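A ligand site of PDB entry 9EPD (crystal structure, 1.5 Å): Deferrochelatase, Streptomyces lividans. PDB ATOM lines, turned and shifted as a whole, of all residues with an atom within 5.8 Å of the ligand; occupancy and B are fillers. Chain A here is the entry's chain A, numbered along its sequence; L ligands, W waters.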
ATOM      1  N   ASN A 186     -38.615 -22.986  11.416  1.00  0.00           N
ATOM      2  CA  ASN A 186     -38.110 -24.349  11.532  1.00  0.00           C
ATOM      3  C   ASN A 186     -38.245 -24.815  12.979  1.00  0.00           C
ATOM      4  O   ASN A 186     -38.668 -24.085  13.854  1.00  0.00           O
ATOM      5  CB  ASN A 186     -36.711 -24.415  10.976  1.00  0.00           C
ATOM      6  CG  ASN A 186     -35.771 -23.473  11.664  1.00  0.00           C
ATOM      7  OD1 ASN A 186     -35.723 -23.411  12.906  1.00  0.00           O
ATOM      8  ND2 ASN A 186     -34.997 -22.760  10.862  1.00  0.00           N
ATOM      9  N   LEU A 188     -36.002 -25.280  15.183  1.00  0.00           N
ATOM     10  CA  LEU A 188     -35.184 -24.540  16.120  1.00  0.00           C
ATOM     11  C   LEU A 188     -35.880 -23.275  16.572  1.00  0.00           C
ATOM     12  O   LEU A 188     -35.352 -22.558  17.398  1.00  0.00           O
ATOM     13  CB  LEU A 188     -33.804 -24.253  15.550  1.00  0.00           C
ATOM     14  CG  LEU A 188     -32.999 -25.448  15.073  1.00  0.00           C
ATOM     15  CD1 LEU A 188     -31.630 -24.975  14.524  1.00  0.00           C
ATOM     16  CD2 LEU A 188     -32.866 -26.543  16.127  1.00  0.00           C
ATOM     17  N   PHE A 190     -36.717 -20.575  14.679  1.00  0.00           N
ATOM     18  CA  PHE A 190     -36.352 -19.403  13.923  1.00  0.00           C
ATOM     19  C   PHE A 190     -37.132 -19.373  12.615  1.00  0.00           C
ATOM     20  O   PHE A 190     -37.270 -20.400  11.933  1.00  0.00           O
ATOM     21  CB  PHE A 190     -34.841 -19.346  13.642  1.00  0.00           C
ATOM     22  CG  PHE A 190     -34.038 -18.797  14.811  1.00  0.00           C
ATOM     23  CD1 PHE A 190     -33.748 -19.588  15.924  1.00  0.00           C
ATOM     24  CD2 PHE A 190     -33.521 -17.503  14.776  1.00  0.00           C
ATOM     25  CE1 PHE A 190     -33.106 -19.051  17.031  1.00  0.00           C
ATOM     26  CE2 PHE A 190     -32.847 -16.984  15.882  1.00  0.00           C
ATOM     27  CZ  PHE A 190     -32.598 -17.765  16.989  1.00  0.00           C
ATOM     28  N   LYS A 191     -37.516 -18.141  12.192  1.00  0.00           N
ATOM     29  CA  LYS A 191     -38.002 -17.946  10.840  1.00  0.00           C
ATOM     30  C   LYS A 191     -36.937 -18.348   9.821  1.00  0.00           C
ATOM     31  O   LYS A 191     -35.772 -18.043  10.000  1.00  0.00           O
ATOM     32  CB  LYS A 191     -38.290 -16.459  10.604  1.00  0.00           C
ATOM     33  CG  LYS A 191     -39.448 -15.931  11.426  1.00  0.00           C
ATOM     34  CD  LYS A 191     -39.686 -14.438  11.160  1.00  0.00           C
ATOM     35  CE  LYS A 191     -40.755 -13.847  11.967  1.00  0.00           C
ATOM     36  NZ  LYS A 191     -40.963 -12.402  11.720  1.00  0.00           N
ATOM     37  N   ASP A 192     -37.372 -19.033   8.769  1.00  0.00           N
ATOM     38  CA  ASP A 192     -36.492 -19.614   7.774  1.00  0.00           C
ATOM     39  C   ASP A 192     -37.147 -19.326   6.420  1.00  0.00           C
ATOM     40  O   ASP A 192     -38.196 -19.867   6.086  1.00  0.00           O
ATOM     41  CB  ASP A 192     -36.319 -21.091   8.061  1.00  0.00           C
ATOM     42  CG  ASP A 192     -35.058 -21.725   7.506  1.00  0.00           C
ATOM     43  OD1 ASP A 192     -34.421 -21.152   6.623  1.00  0.00           O
ATOM     44  OD2 ASP A 192     -34.747 -22.817   7.992  1.00  0.00           O
ATOM     45  N   GLY A 193     -36.499 -18.467   5.654  1.00  0.00           N
ATOM     46  CA  GLY A 193     -36.965 -18.100   4.331  1.00  0.00           C
ATOM     47  C   GLY A 193     -37.025 -16.592   4.074  1.00  0.00           C
ATOM     48  O   GLY A 193     -37.440 -16.223   2.997  1.00  0.00           O
ATOM     49  N   THR A 194     -36.579 -15.751   5.000  1.00  0.00           N
ATOM     50  CA  THR A 194     -36.671 -14.302   4.866  1.00  0.00           C
ATOM     51  C   THR A 194     -35.955 -13.820   3.618  1.00  0.00           C
ATOM     52  O   THR A 194     -36.562 -13.085   2.806  1.00  0.00           O
ATOM     53  CB  THR A 194     -36.124 -13.652   6.130  1.00  0.00           C
ATOM     54  OG1 THR A 194     -36.871 -14.125   7.256  1.00  0.00           O
ATOM     55  CG2 THR A 194     -36.142 -12.142   5.939  1.00  0.00           C
ATOM     56  N   ARG A 195     -34.689 -14.202   3.454  1.00  0.00           N
ATOM     57  CA  ARG A 195     -33.938 -13.719   2.314  1.00  0.00           C
ATOM     58  C   ARG A 195     -33.728 -14.880   1.367  1.00  0.00           C
ATOM     59  O   ARG A 195     -32.687 -15.538   1.394  1.00  0.00           O
ATOM     60  CB  ARG A 195     -32.636 -13.064   2.799  1.00  0.00           C
ATOM     61  CG  ARG A 195     -32.785 -11.624   3.246  1.00  0.00           C
ATOM     62  CD  ARG A 195     -31.526 -10.906   3.674  1.00  0.00           C
ATOM     63  NE  ARG A 195     -30.379 -11.236   2.838  1.00  0.00           N
ATOM     64  CZ  ARG A 195     -30.191 -10.882   1.592  1.00  0.00           C
ATOM     65  NH1 ARG A 195     -29.376 -11.585   0.834  1.00  0.00           N
ATOM     66  NH2 ARG A 195     -30.844  -9.868   1.063  1.00  0.00           N
ATOM     67  N   ASN A 196     -34.723 -15.107   0.540  1.00  0.00           N
ATOM     68  CA  ASN A 196     -34.735 -16.170  -0.437  1.00  0.00           C
ATOM     69  C   ASN A 196     -34.866 -15.480  -1.779  1.00  0.00           C
ATOM     70  O   ASN A 196     -34.265 -14.432  -2.010  1.00  0.00           O
ATOM     71  CB  ASN A 196     -35.754 -17.218  -0.017  1.00  0.00           C
ATOM     72  CG  ASN A 196     -35.610 -18.542  -0.735  1.00  0.00           C
ATOM     73  OD1 ASN A 196     -34.500 -18.933  -0.993  1.00  0.00           O
ATOM     74  ND2 ASN A 196     -36.681 -19.171  -1.200  1.00  0.00           N
ATOM     75  N   ILE A 231     -31.138 -33.304   7.045  1.00  0.00           N
ATOM     76  CA  ILE A 231     -30.327 -32.804   8.136  1.00  0.00           C
ATOM     77  C   ILE A 231     -31.013 -33.105   9.453  1.00  0.00           C
ATOM     78  O   ILE A 231     -32.108 -32.615   9.721  1.00  0.00           O
ATOM     79  CB  ILE A 231     -30.102 -31.286   7.993  1.00  0.00           C
ATOM     80  CG1 ILE A 231     -29.549 -30.985   6.635  1.00  0.00           C
ATOM     81  CG2 ILE A 231     -29.208 -30.780   9.131  1.00  0.00           C
ATOM     82  CD1 ILE A 231     -29.303 -29.513   6.339  1.00  0.00           C
ATOM     83  N   MET A 233     -31.403 -32.550  13.393  1.00  0.00           N
ATOM     84  CA  MET A 233     -31.191 -31.526  14.399  1.00  0.00           C
ATOM     85  C   MET A 233     -31.020 -32.134  15.790  1.00  0.00           C
ATOM     86  O   MET A 233     -31.798 -32.994  16.219  1.00  0.00           O
ATOM     87  CB  MET A 233     -32.383 -30.562  14.479  1.00  0.00           C
ATOM     88  CG  MET A 233     -32.506 -29.719  13.266  1.00  0.00           C
ATOM     89  SD  MET A 233     -34.118 -28.904  13.183  1.00  0.00           S
ATOM     90  CE  MET A 233     -33.663 -27.599  12.051  1.00  0.00           C
ATOM     91  N   PHE A 250     -27.254 -17.649  14.660  1.00  0.00           N
ATOM     92  CA  PHE A 250     -27.868 -17.211  13.408  1.00  0.00           C
ATOM     93  C   PHE A 250     -27.484 -15.805  12.976  1.00  0.00           C
ATOM     94  O   PHE A 250     -27.281 -15.566  11.791  1.00  0.00           O
ATOM     95  CB  PHE A 250     -29.394 -17.352  13.431  1.00  0.00           C
ATOM     96  CG  PHE A 250     -29.799 -18.800  13.272  1.00  0.00           C
ATOM     97  CD1 PHE A 250     -29.516 -19.504  12.113  1.00  0.00           C
ATOM     98  CD2 PHE A 250     -30.383 -19.471  14.329  1.00  0.00           C
ATOM     99  CE1 PHE A 250     -29.844 -20.831  12.014  1.00  0.00           C
ATOM    100  CE2 PHE A 250     -30.690 -20.816  14.217  1.00  0.00           C
ATOM    101  CZ  PHE A 250     -30.434 -21.473  13.061  1.00  0.00           C
ATOM    102  N   ARG A 252     -29.625 -13.346  13.771  1.00  0.00           N
ATOM    103  CA  ARG A 252     -30.932 -12.714  13.816  1.00  0.00           C
ATOM    104  C   ARG A 252     -31.561 -13.004  15.165  1.00  0.00           C
ATOM    105  O   ARG A 252     -31.166 -13.984  15.842  1.00  0.00           O
ATOM    106  CB  ARG A 252     -31.839 -13.250  12.719  1.00  0.00           C
ATOM    107  CG  ARG A 252     -31.458 -12.796  11.327  1.00  0.00           C
ATOM    108  CD  ARG A 252     -32.357 -13.458  10.273  1.00  0.00           C
ATOM    109  NE  ARG A 252     -32.086 -13.008   8.916  1.00  0.00           N
ATOM    110  CZ  ARG A 252     -32.664 -11.952   8.347  1.00  0.00           C
ATOM    111  NH1 ARG A 252     -33.546 -11.177   8.981  1.00  0.00           N
ATOM    112  NH2 ARG A 252     -32.337 -11.718   7.110  1.00  0.00           N
ATOM    113  N   PRO A 269     -29.517  -7.251   6.551  1.00  0.00           N
ATOM    114  CA  PRO A 269     -28.473  -7.547   7.514  1.00  0.00           C
ATOM    115  C   PRO A 269     -27.286  -6.623   7.339  1.00  0.00           C
ATOM    116  O   PRO A 269     -26.838  -6.350   6.236  1.00  0.00           O
ATOM    117  CB  PRO A 269     -28.070  -8.955   7.225  1.00  0.00           C
ATOM    118  CG  PRO A 269     -28.691  -9.312   5.974  1.00  0.00           C
ATOM    119  CD  PRO A 269     -29.802  -8.369   5.645  1.00  0.00           C
ATOM    120  N   HIS A 279     -24.482 -18.121  11.101  1.00  0.00           N
ATOM    121  CA  HIS A 279     -24.961 -18.779   9.899  1.00  0.00           C
ATOM    122  C   HIS A 279     -25.318 -17.769   8.792  1.00  0.00           C
ATOM    123  O   HIS A 279     -24.983 -17.976   7.650  1.00  0.00           O
ATOM    124  CB  HIS A 279     -26.203 -19.588  10.274  1.00  0.00           C
ATOM    125  CG  HIS A 279     -26.831 -20.317   9.126  1.00  0.00           C
ATOM    126  ND1 HIS A 279     -26.269 -21.442   8.607  1.00  0.00           N
ATOM    127  CD2 HIS A 279     -28.018 -20.176   8.468  1.00  0.00           C
ATOM    128  CE1 HIS A 279     -27.052 -21.908   7.623  1.00  0.00           C
ATOM    129  NE2 HIS A 279     -28.120 -21.153   7.539  1.00  0.00           N
ATOM    130  N   VAL A 280     -26.101 -16.743   9.116  1.00  0.00           N
ATOM    131  CA  VAL A 280     -26.498 -15.766   8.111  1.00  0.00           C
ATOM    132  C   VAL A 280     -25.274 -15.088   7.525  1.00  0.00           C
ATOM    133  O   VAL A 280     -25.182 -14.902   6.317  1.00  0.00           O
ATOM    134  CB  VAL A 280     -27.519 -14.765   8.658  1.00  0.00           C
ATOM    135  CG1 VAL A 280     -27.760 -13.652   7.663  1.00  0.00           C
ATOM    136  CG2 VAL A 280     -28.822 -15.476   8.996  1.00  0.00           C
ATOM    137  N   ALA A 283     -23.592 -17.604   5.159  1.00  0.00           N
ATOM    138  CA  ALA A 283     -24.438 -18.062   4.072  1.00  0.00           C
ATOM    139  C   ALA A 283     -24.809 -16.965   3.082  1.00  0.00           C
ATOM    140  O   ALA A 283     -25.243 -17.277   1.969  1.00  0.00           O
ATOM    141  CB  ALA A 283     -25.676 -18.704   4.614  1.00  0.00           C
ATOM    142  N   HIS A 284     -24.634 -15.715   3.480  1.00  0.00           N
ATOM    143  CA  HIS A 284     -25.147 -14.566   2.727  1.00  0.00           C
ATOM    144  C   HIS A 284     -24.437 -14.455   1.391  1.00  0.00           C
ATOM    145  O   HIS A 284     -23.237 -14.726   1.301  1.00  0.00           O
ATOM    146  CB  HIS A 284     -24.879 -13.279   3.522  1.00  0.00           C
ATOM    147  CG  HIS A 284     -25.567 -12.060   3.005  1.00  0.00           C
ATOM    148  ND1 HIS A 284     -25.103 -11.348   1.925  1.00  0.00           N
ATOM    149  CD2 HIS A 284     -26.679 -11.409   3.430  1.00  0.00           C
ATOM    150  CE1 HIS A 284     -25.917 -10.312   1.714  1.00  0.00           C
ATOM    151  NE2 HIS A 284     -26.851 -10.297   2.641  1.00  0.00           N
ATOM    152  N   PRO A 285     -25.120 -14.086   0.294  1.00  0.00           N
ATOM    153  CA  PRO A 285     -24.451 -13.978  -1.013  1.00  0.00           C
ATOM    154  C   PRO A 285     -23.199 -13.104  -0.975  1.00  0.00           C
ATOM    155  O   PRO A 285     -22.216 -13.453  -1.627  1.00  0.00           O
ATOM    156  CB  PRO A 285     -25.557 -13.403  -1.927  1.00  0.00           C
ATOM    157  CG  PRO A 285     -26.797 -13.843  -1.305  1.00  0.00           C
ATOM    158  CD  PRO A 285     -26.560 -13.839   0.193  1.00  0.00           C
ATOM    159  N   LEU A 293     -29.219 -18.880  -3.675  1.00  0.00           N
ATOM    160  CA  LEU A 293     -29.972 -20.124  -3.835  1.00  0.00           C
ATOM    161  C   LEU A 293     -31.442 -19.873  -3.685  1.00  0.00           C
ATOM    162  O   LEU A 293     -31.823 -18.932  -3.005  1.00  0.00           O
ATOM    163  CB  LEU A 293     -29.625 -21.086  -2.681  1.00  0.00           C
ATOM    164  CG  LEU A 293     -28.156 -21.386  -2.476  1.00  0.00           C
ATOM    165  CD1 LEU A 293     -28.015 -22.164  -1.188  1.00  0.00           C
ATOM    166  CD2 LEU A 293     -27.748 -22.247  -3.636  1.00  0.00           C
ATOM    167  N   ARG A 295     -34.126 -21.678  -1.756  1.00  0.00           N
ATOM    168  CA  ARG A 295     -34.313 -22.683  -0.725  1.00  0.00           C
ATOM    169  C   ARG A 295     -35.793 -23.009  -0.615  1.00  0.00           C
ATOM    170  O   ARG A 295     -36.623 -22.126  -0.617  1.00  0.00           O
ATOM    171  CB  ARG A 295     -33.861 -22.131   0.628  1.00  0.00           C
ATOM    172  CG  ARG A 295     -32.353 -21.994   0.721  1.00  0.00           C
ATOM    173  CD  ARG A 295     -31.969 -21.321   1.985  1.00  0.00           C
ATOM    174  NE  ARG A 295     -32.301 -19.893   1.987  1.00  0.00           N
ATOM    175  CZ  ARG A 295     -32.766 -19.239   3.022  1.00  0.00           C
ATOM    176  NH1 ARG A 295     -33.026 -19.853   4.159  1.00  0.00           N
ATOM    177  NH2 ARG A 295     -33.075 -17.958   2.895  1.00  0.00           N
ATOM    178  N   LEU A 314     -34.547 -31.280   9.261  1.00  0.00           N
ATOM    179  CA  LEU A 314     -34.932 -30.398   8.184  1.00  0.00           C
ATOM    180  C   LEU A 314     -34.519 -31.091   6.905  1.00  0.00           C
ATOM    181  O   LEU A 314     -33.387 -31.481   6.744  1.00  0.00           O
ATOM    182  CB  LEU A 314     -34.301 -29.025   8.429  1.00  0.00           C
ATOM    183  CG  LEU A 314     -34.850 -27.903   7.533  1.00  0.00           C
ATOM    184  CD1 LEU A 314     -34.801 -26.588   8.270  1.00  0.00           C
ATOM    185  CD2 LEU A 314     -34.076 -27.832   6.248  1.00  0.00           C
ATOM    186  N   PHE A 316     -33.643 -30.209   3.578  1.00  0.00           N
ATOM    187  CA  PHE A 316     -33.183 -29.025   2.899  1.00  0.00           C
ATOM    188  C   PHE A 316     -33.229 -29.284   1.396  1.00  0.00           C
ATOM    189  O   PHE A 316     -32.671 -30.288   0.942  1.00  0.00           O
ATOM    190  CB  PHE A 316     -31.757 -28.764   3.410  1.00  0.00           C
ATOM    191  CG  PHE A 316     -31.221 -27.500   2.785  1.00  0.00           C
ATOM    192  CD1 PHE A 316     -31.469 -26.263   3.376  1.00  0.00           C
ATOM    193  CD2 PHE A 316     -30.428 -27.532   1.652  1.00  0.00           C
ATOM    194  CE1 PHE A 316     -30.941 -25.110   2.829  1.00  0.00           C
ATOM    195  CE2 PHE A 316     -29.911 -26.380   1.115  1.00  0.00           C
ATOM    196  CZ  PHE A 316     -30.192 -25.167   1.701  1.00  0.00           C
ATOM    197  N   PHE A 327     -25.018 -24.295  -4.406  1.00  0.00           N
ATOM    198  CA  PHE A 327     -24.919 -24.981  -3.131  1.00  0.00           C
ATOM    199  C   PHE A 327     -23.464 -25.148  -2.686  1.00  0.00           C
ATOM    200  O   PHE A 327     -23.185 -25.016  -1.502  1.00  0.00           O
ATOM    201  CB  PHE A 327     -25.627 -26.333  -3.230  1.00  0.00           C
ATOM    202  CG  PHE A 327     -25.570 -27.167  -1.951  1.00  0.00           C
ATOM    203  CD1 PHE A 327     -26.397 -26.903  -0.867  1.00  0.00           C
ATOM    204  CD2 PHE A 327     -24.614 -28.183  -1.821  1.00  0.00           C
ATOM    205  CE1 PHE A 327     -26.291 -27.623   0.304  1.00  0.00           C
ATOM    206  CE2 PHE A 327     -24.503 -28.865  -0.620  1.00  0.00           C
ATOM    207  CZ  PHE A 327     -25.341 -28.611   0.424  1.00  0.00           C
ATOM    208  N   VAL A 330     -21.537 -22.227  -1.072  1.00  0.00           N
ATOM    209  CA  VAL A 330     -22.159 -21.806   0.155  1.00  0.00           C
ATOM    210  C   VAL A 330     -21.909 -22.856   1.236  1.00  0.00           C
ATOM    211  O   VAL A 330     -21.532 -22.504   2.353  1.00  0.00           O
ATOM    212  CB  VAL A 330     -23.632 -21.461  -0.055  1.00  0.00           C
ATOM    213  CG1 VAL A 330     -24.256 -21.139   1.269  1.00  0.00           C
ATOM    214  CG2 VAL A 330     -23.798 -20.297  -1.040  1.00  0.00           C
ATOM    215  N   GLN A 331     -22.152 -24.109   0.939  1.00  0.00           N
ATOM    216  CA  GLN A 331     -21.939 -25.147   1.950  1.00  0.00           C
ATOM    217  C   GLN A 331     -20.474 -25.196   2.367  1.00  0.00           C
ATOM    218  O   GLN A 331     -20.172 -25.448   3.543  1.00  0.00           O
ATOM    219  CB  GLN A 331     -22.386 -26.512   1.432  1.00  0.00           C
ATOM    220  CG  GLN A 331     -22.191 -27.666   2.426  1.00  0.00           C
ATOM    221  CD  GLN A 331     -22.951 -27.535   3.730  1.00  0.00           C
ATOM    222  OE1 GLN A 331     -24.057 -27.022   3.820  1.00  0.00           O
ATOM    223  NE2 GLN A 331     -22.379 -28.058   4.797  1.00  0.00           N
ATOM    224  N   LEU A 334     -19.839 -22.863   5.039  1.00  0.00           N
ATOM    225  CA  LEU A 334     -20.439 -23.198   6.321  1.00  0.00           C
ATOM    226  C   LEU A 334     -19.575 -24.187   7.091  1.00  0.00           C
ATOM    227  O   LEU A 334     -19.979 -24.602   8.172  1.00  0.00           O
ATOM    228  CB  LEU A 334     -21.836 -23.760   6.072  1.00  0.00           C
ATOM    229  CG  LEU A 334     -22.852 -22.827   5.404  1.00  0.00           C
ATOM    230  CD1 LEU A 334     -24.280 -23.433   5.380  1.00  0.00           C
ATOM    231  CD2 LEU A 334     -22.793 -21.532   6.138  1.00  0.00           C
ATOM    232  N   LEU A 339     -23.774 -23.121  13.618  1.00  0.00           N
ATOM    233  CA  LEU A 339     -24.904 -24.034  13.540  1.00  0.00           C
ATOM    234  C   LEU A 339     -24.438 -25.483  13.491  1.00  0.00           C
ATOM    235  O   LEU A 339     -25.192 -26.398  13.866  1.00  0.00           O
ATOM    236  CB  LEU A 339     -25.720 -23.664  12.304  1.00  0.00           C
ATOM    237  CG  LEU A 339     -27.001 -24.495  12.134  1.00  0.00           C
ATOM    238  CD1 LEU A 339     -28.014 -24.344  13.252  1.00  0.00           C
ATOM    239  CD2 LEU A 339     -27.621 -24.144  10.793  1.00  0.00           C
ATOM    240  N   ILE A 343     -26.415 -29.694  14.200  1.00  0.00           N
ATOM    241  CA  ILE A 343     -26.996 -30.400  13.069  1.00  0.00           C
ATOM    242  C   ILE A 343     -26.018 -31.441  12.554  1.00  0.00           C
ATOM    243  O   ILE A 343     -24.806 -31.379  12.829  1.00  0.00           O
ATOM    244  CB  ILE A 343     -27.332 -29.417  11.920  1.00  0.00           C
ATOM    245  CG1 ILE A 343     -26.065 -28.798  11.304  1.00  0.00           C
ATOM    246  CG2 ILE A 343     -28.372 -28.353  12.306  1.00  0.00           C
ATOM    247  CD1 ILE A 343     -26.325 -28.102   9.992  1.00  0.00           C
ATOM    248  N   HIS A 345     -25.672 -33.614   8.625  1.00  0.00           N
ATOM    249  CA  HIS A 345     -26.200 -34.001   7.338  1.00  0.00           C
ATOM    250  C   HIS A 345     -26.095 -35.515   7.252  1.00  0.00           C
ATOM    251  O   HIS A 345     -24.999 -36.043   7.399  1.00  0.00           O
ATOM    252  CB  HIS A 345     -25.422 -33.360   6.211  1.00  0.00           C
ATOM    253  CG  HIS A 345     -25.567 -31.876   6.093  1.00  0.00           C
ATOM    254  ND1 HIS A 345     -25.887 -31.230   4.909  1.00  0.00           N
ATOM    255  CD2 HIS A 345     -25.369 -30.911   7.001  1.00  0.00           C
ATOM    256  CE1 HIS A 345     -25.902 -29.925   5.147  1.00  0.00           C
ATOM    257  NE2 HIS A 345     -25.558 -29.708   6.413  1.00  0.00           N
HETATM  258  C1  LIG L   1     -30.697 -18.278   6.193  1.00  0.00           C
HETATM  259  C2  LIG L   1     -31.686 -21.760   9.368  1.00  0.00           C
HETATM  260  C3  LIG L   1     -29.241 -24.978   6.620  1.00  0.00           C
HETATM  261  C4  LIG L   1     -28.377 -21.440   3.438  1.00  0.00           C
HETATM  262  C5  LIG L   1     -31.162 -18.900   7.317  1.00  0.00           C
HETATM  263  C6  LIG L   1     -31.857 -18.308   8.365  1.00  0.00           C
HETATM  264  C7  LIG L   1     -32.171 -19.304   9.236  1.00  0.00           C
HETATM  265  C8  LIG L   1     -31.576 -20.521   8.749  1.00  0.00           C
HETATM  266  C9  LIG L   1     -32.878 -19.121  10.557  1.00  0.00           C
HETATM  267  C10 LIG L   1     -32.241 -16.848   8.469  1.00  0.00           C
HETATM  268  C11 LIG L   1     -33.502 -16.470   7.746  1.00  0.00           C
HETATM  269  C12 LIG L   1     -33.425 -16.553   6.278  1.00  0.00           C
HETATM  270  O1  LIG L   1     -33.921 -17.574   5.736  1.00  0.00           O
HETATM  271  O2  LIG L   1     -33.005 -15.631   5.557  1.00  0.00           O
HETATM  272  C13 LIG L   1     -31.110 -22.948   8.860  1.00  0.00           C
HETATM  273  C14 LIG L   1     -31.231 -24.230   9.482  1.00  0.00           C
HETATM  274  C15 LIG L   1     -30.533 -25.094   8.716  1.00  0.00           C
HETATM  275  C16 LIG L   1     -29.961 -24.371   7.619  1.00  0.00           C
HETATM  276  C17 LIG L   1     -31.988 -24.454  10.756  1.00  0.00           C
HETATM  277  C18 LIG L   1     -30.324 -26.560   8.875  1.00  0.00           C
HETATM  278  C19 LIG L   1     -31.010 -27.318   9.711  1.00  0.00           C
HETATM  279  C20 LIG L   1     -28.769 -24.298   5.541  1.00  0.00           C
HETATM  280  C21 LIG L   1     -27.990 -24.831   4.511  1.00  0.00           C
HETATM  281  C22 LIG L   1     -27.732 -23.830   3.582  1.00  0.00           C
HETATM  282  C23 LIG L   1     -28.394 -22.677   4.074  1.00  0.00           C
HETATM  283  C24 LIG L   1     -27.564 -26.248   4.481  1.00  0.00           C
HETATM  284  C25 LIG L   1     -26.923 -23.830   2.344  1.00  0.00           C
HETATM  285  C26 LIG L   1     -26.084 -24.715   2.009  1.00  0.00           C
HETATM  286  C27 LIG L   1     -28.986 -20.279   3.931  1.00  0.00           C
HETATM  287  C28 LIG L   1     -28.962 -19.040   3.158  1.00  0.00           C
HETATM  288  C29 LIG L   1     -29.593 -18.141   3.970  1.00  0.00           C
HETATM  289  C30 LIG L   1     -30.009 -18.873   5.177  1.00  0.00           C
HETATM  290  C31 LIG L   1     -28.382 -18.833   1.769  1.00  0.00           C
HETATM  291  C32 LIG L   1     -29.829 -16.682   3.546  1.00  0.00           C
HETATM  292  C33 LIG L   1     -28.707 -15.753   3.936  1.00  0.00           C
HETATM  293  C34 LIG L   1     -28.957 -14.346   3.529  1.00  0.00           C
HETATM  294  O3  LIG L   1     -29.343 -13.507   4.370  1.00  0.00           O
HETATM  295  O4  LIG L   1     -28.861 -14.092   2.298  1.00  0.00           O
HETATM  296  N1  LIG L   1     -30.980 -20.301   7.559  1.00  0.00           N
HETATM  297  N2  LIG L   1     -30.409 -23.080   7.743  1.00  0.00           N
HETATM  298  N3  LIG L   1     -28.983 -22.944   5.291  1.00  0.00           N
HETATM  299  N4  LIG L   1     -29.594 -20.177   5.108  1.00  0.00           N
HETATM  300 FE1  LIG L   1     -29.879 -21.553   6.457  1.00  0.00          FE
HETATM  301  O   HOH W   1     -29.110 -17.303  -1.192  1.00  0.00           O
HETATM  302  O   HOH W   2     -30.958 -14.026   6.385  1.00  0.00           O
HETATM  303  O   HOH W   3     -26.419 -17.544  -0.541  1.00  0.00           O
HETATM  304  O   HOH W   4     -30.236 -15.116   0.133  1.00  0.00           O
HETATM  305  O   HOH W   5     -25.030 -27.031   6.613  1.00  0.00           O
HETATM  306  O   HOH W   6     -33.155 -24.332   6.414  1.00  0.00           O
HETATM  307  O   HOH W   7     -31.999 -22.067   5.596  1.00  0.00           O
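A ring nitrogen (NE2) of His 279 is bound to an iron atom (FE1) of the ligand (2.1 Å).
The backbone NH (N) of Gly 193 sits at hydrogen-bond distance from an oxygen (O1) of the ligand.
The guanidinium group (NH1) of Arg 295 is in salt-bridge range of an oxygen (O1) of the ligand.
N of Arg 195 sits at hydrogen-bond distance from O2 of the ligand.
The guanidinium group (NE) of Arg 195 lies within salt-bridge range of an oxygen (O3) of the ligand, at 2.9 Å.
An oxygen (O1) of the ligand lies within hydrogen-bond range of the backbone NH of Thr 194 (3.3 Å).
The guanidinium group (NH2) of Arg 295 sits at hydrogen-bond distance from the backbone carbonyl oxygen (O) of Arg 195.
NH1 of Arg 295 lies within salt-bridge range of OD1 of Asp 192, at 3.1 Å.
The backbone NH of Arg 295 lies within hydrogen-bond range of the side-chain amide oxygen of Asn 196, at 2.9 Å.
NH1 of Arg 195 lies within hydrogen-bond range of NE2 of His 284, 3.4 Å away.
The backbone carbonyl oxygen (O) of Phe 250 is in hydrogen-bond range of the backbone NH (N) of Val 280 (3.2 Å).
The side-chain amide nitrogen of Asn 186 lies close to the backbone carbonyl oxygen of Phe 190.
The side-chain amide oxygen of Asn 186 sits at hydrogen-bond distance from the backbone NH of Leu 188, at 3.0 Å.
O of Ile 231 is in hydrogen-bond range of N of Leu 314 (2.8 Å).
Asn 186 touches the ligand (ND2 to C17, 3.5 Å).
CD1 of Leu 188 touches C17 of the ligand, at 3.8 Å.
Phe 190 touches the ligand.
Lys 191 touches the ligand (O to C9, 3.1 Å).
Asp 192 touches the ligand.
Ile 231 touches the ligand (CG2 to C19, 3.9 Å).
CE of Met 233 touches C19 of the ligand (3.5 Å).
Phe 250 touches the ligand.
Arg 252 touches the ligand (CD to C10, 3.8 Å).
Val 280 touches the ligand.
O of Ala 283 touches C31 of the ligand, 3.5 Å away.
His 284 touches the ligand (CD2 to O3, 3.5 Å).
Pro 285 touches the ligand (CD to O4, 3.1 Å).
Leu 314 touches the ligand (CB to C19, 3.9 Å).
Phe 316 touches the ligand (CZ to C22, 3.4 Å).
CE1 of Phe 327 touches C26 of the ligand, at 3.4 Å.
Val 330 touches the ligand.
Gln 331 touches the ligand (OE1 to C26, 3.6 Å).
CD1 of Leu 334 touches C22 of the ligand, at 3.9 Å.
Leu 339 touches the ligand.
Ile 343 touches the ligand.
Hydrophobic or aromatic side chains that line the ligand: Leu 188, Phe 190, Ile 231, Met 233, Phe 250, His 279, Val 280, Ala 283, His 284, Pro 285, Leu 314, Phe 316, Phe 327, Val 330, Leu 334, Leu 339 and Ile 343.
Of the 30 residues printed, 26 come within 4 Å of the ligand.
The nearest printed residue that does not touch the ligand is Leu 293 (4.1 Å).
Water W7 lies within hydrogen-bond range of OD1 of Asp 192 (2.8 Å) and NH1 of Arg 295 (2.8 Å).
Water W2 lies within hydrogen-bond range of O3 of the ligand (2.6 Å) and NH2 of Arg 252 (2.8 Å).
Water W4 lies within hydrogen-bond range of O4 of the ligand (2.8 Å) and O of Arg 195 (2.8 Å).
Water W5 lies within hydrogen-bond range of a ring nitrogen (NE2) of His 345 and the side-chain amide oxygen of Gln 331.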
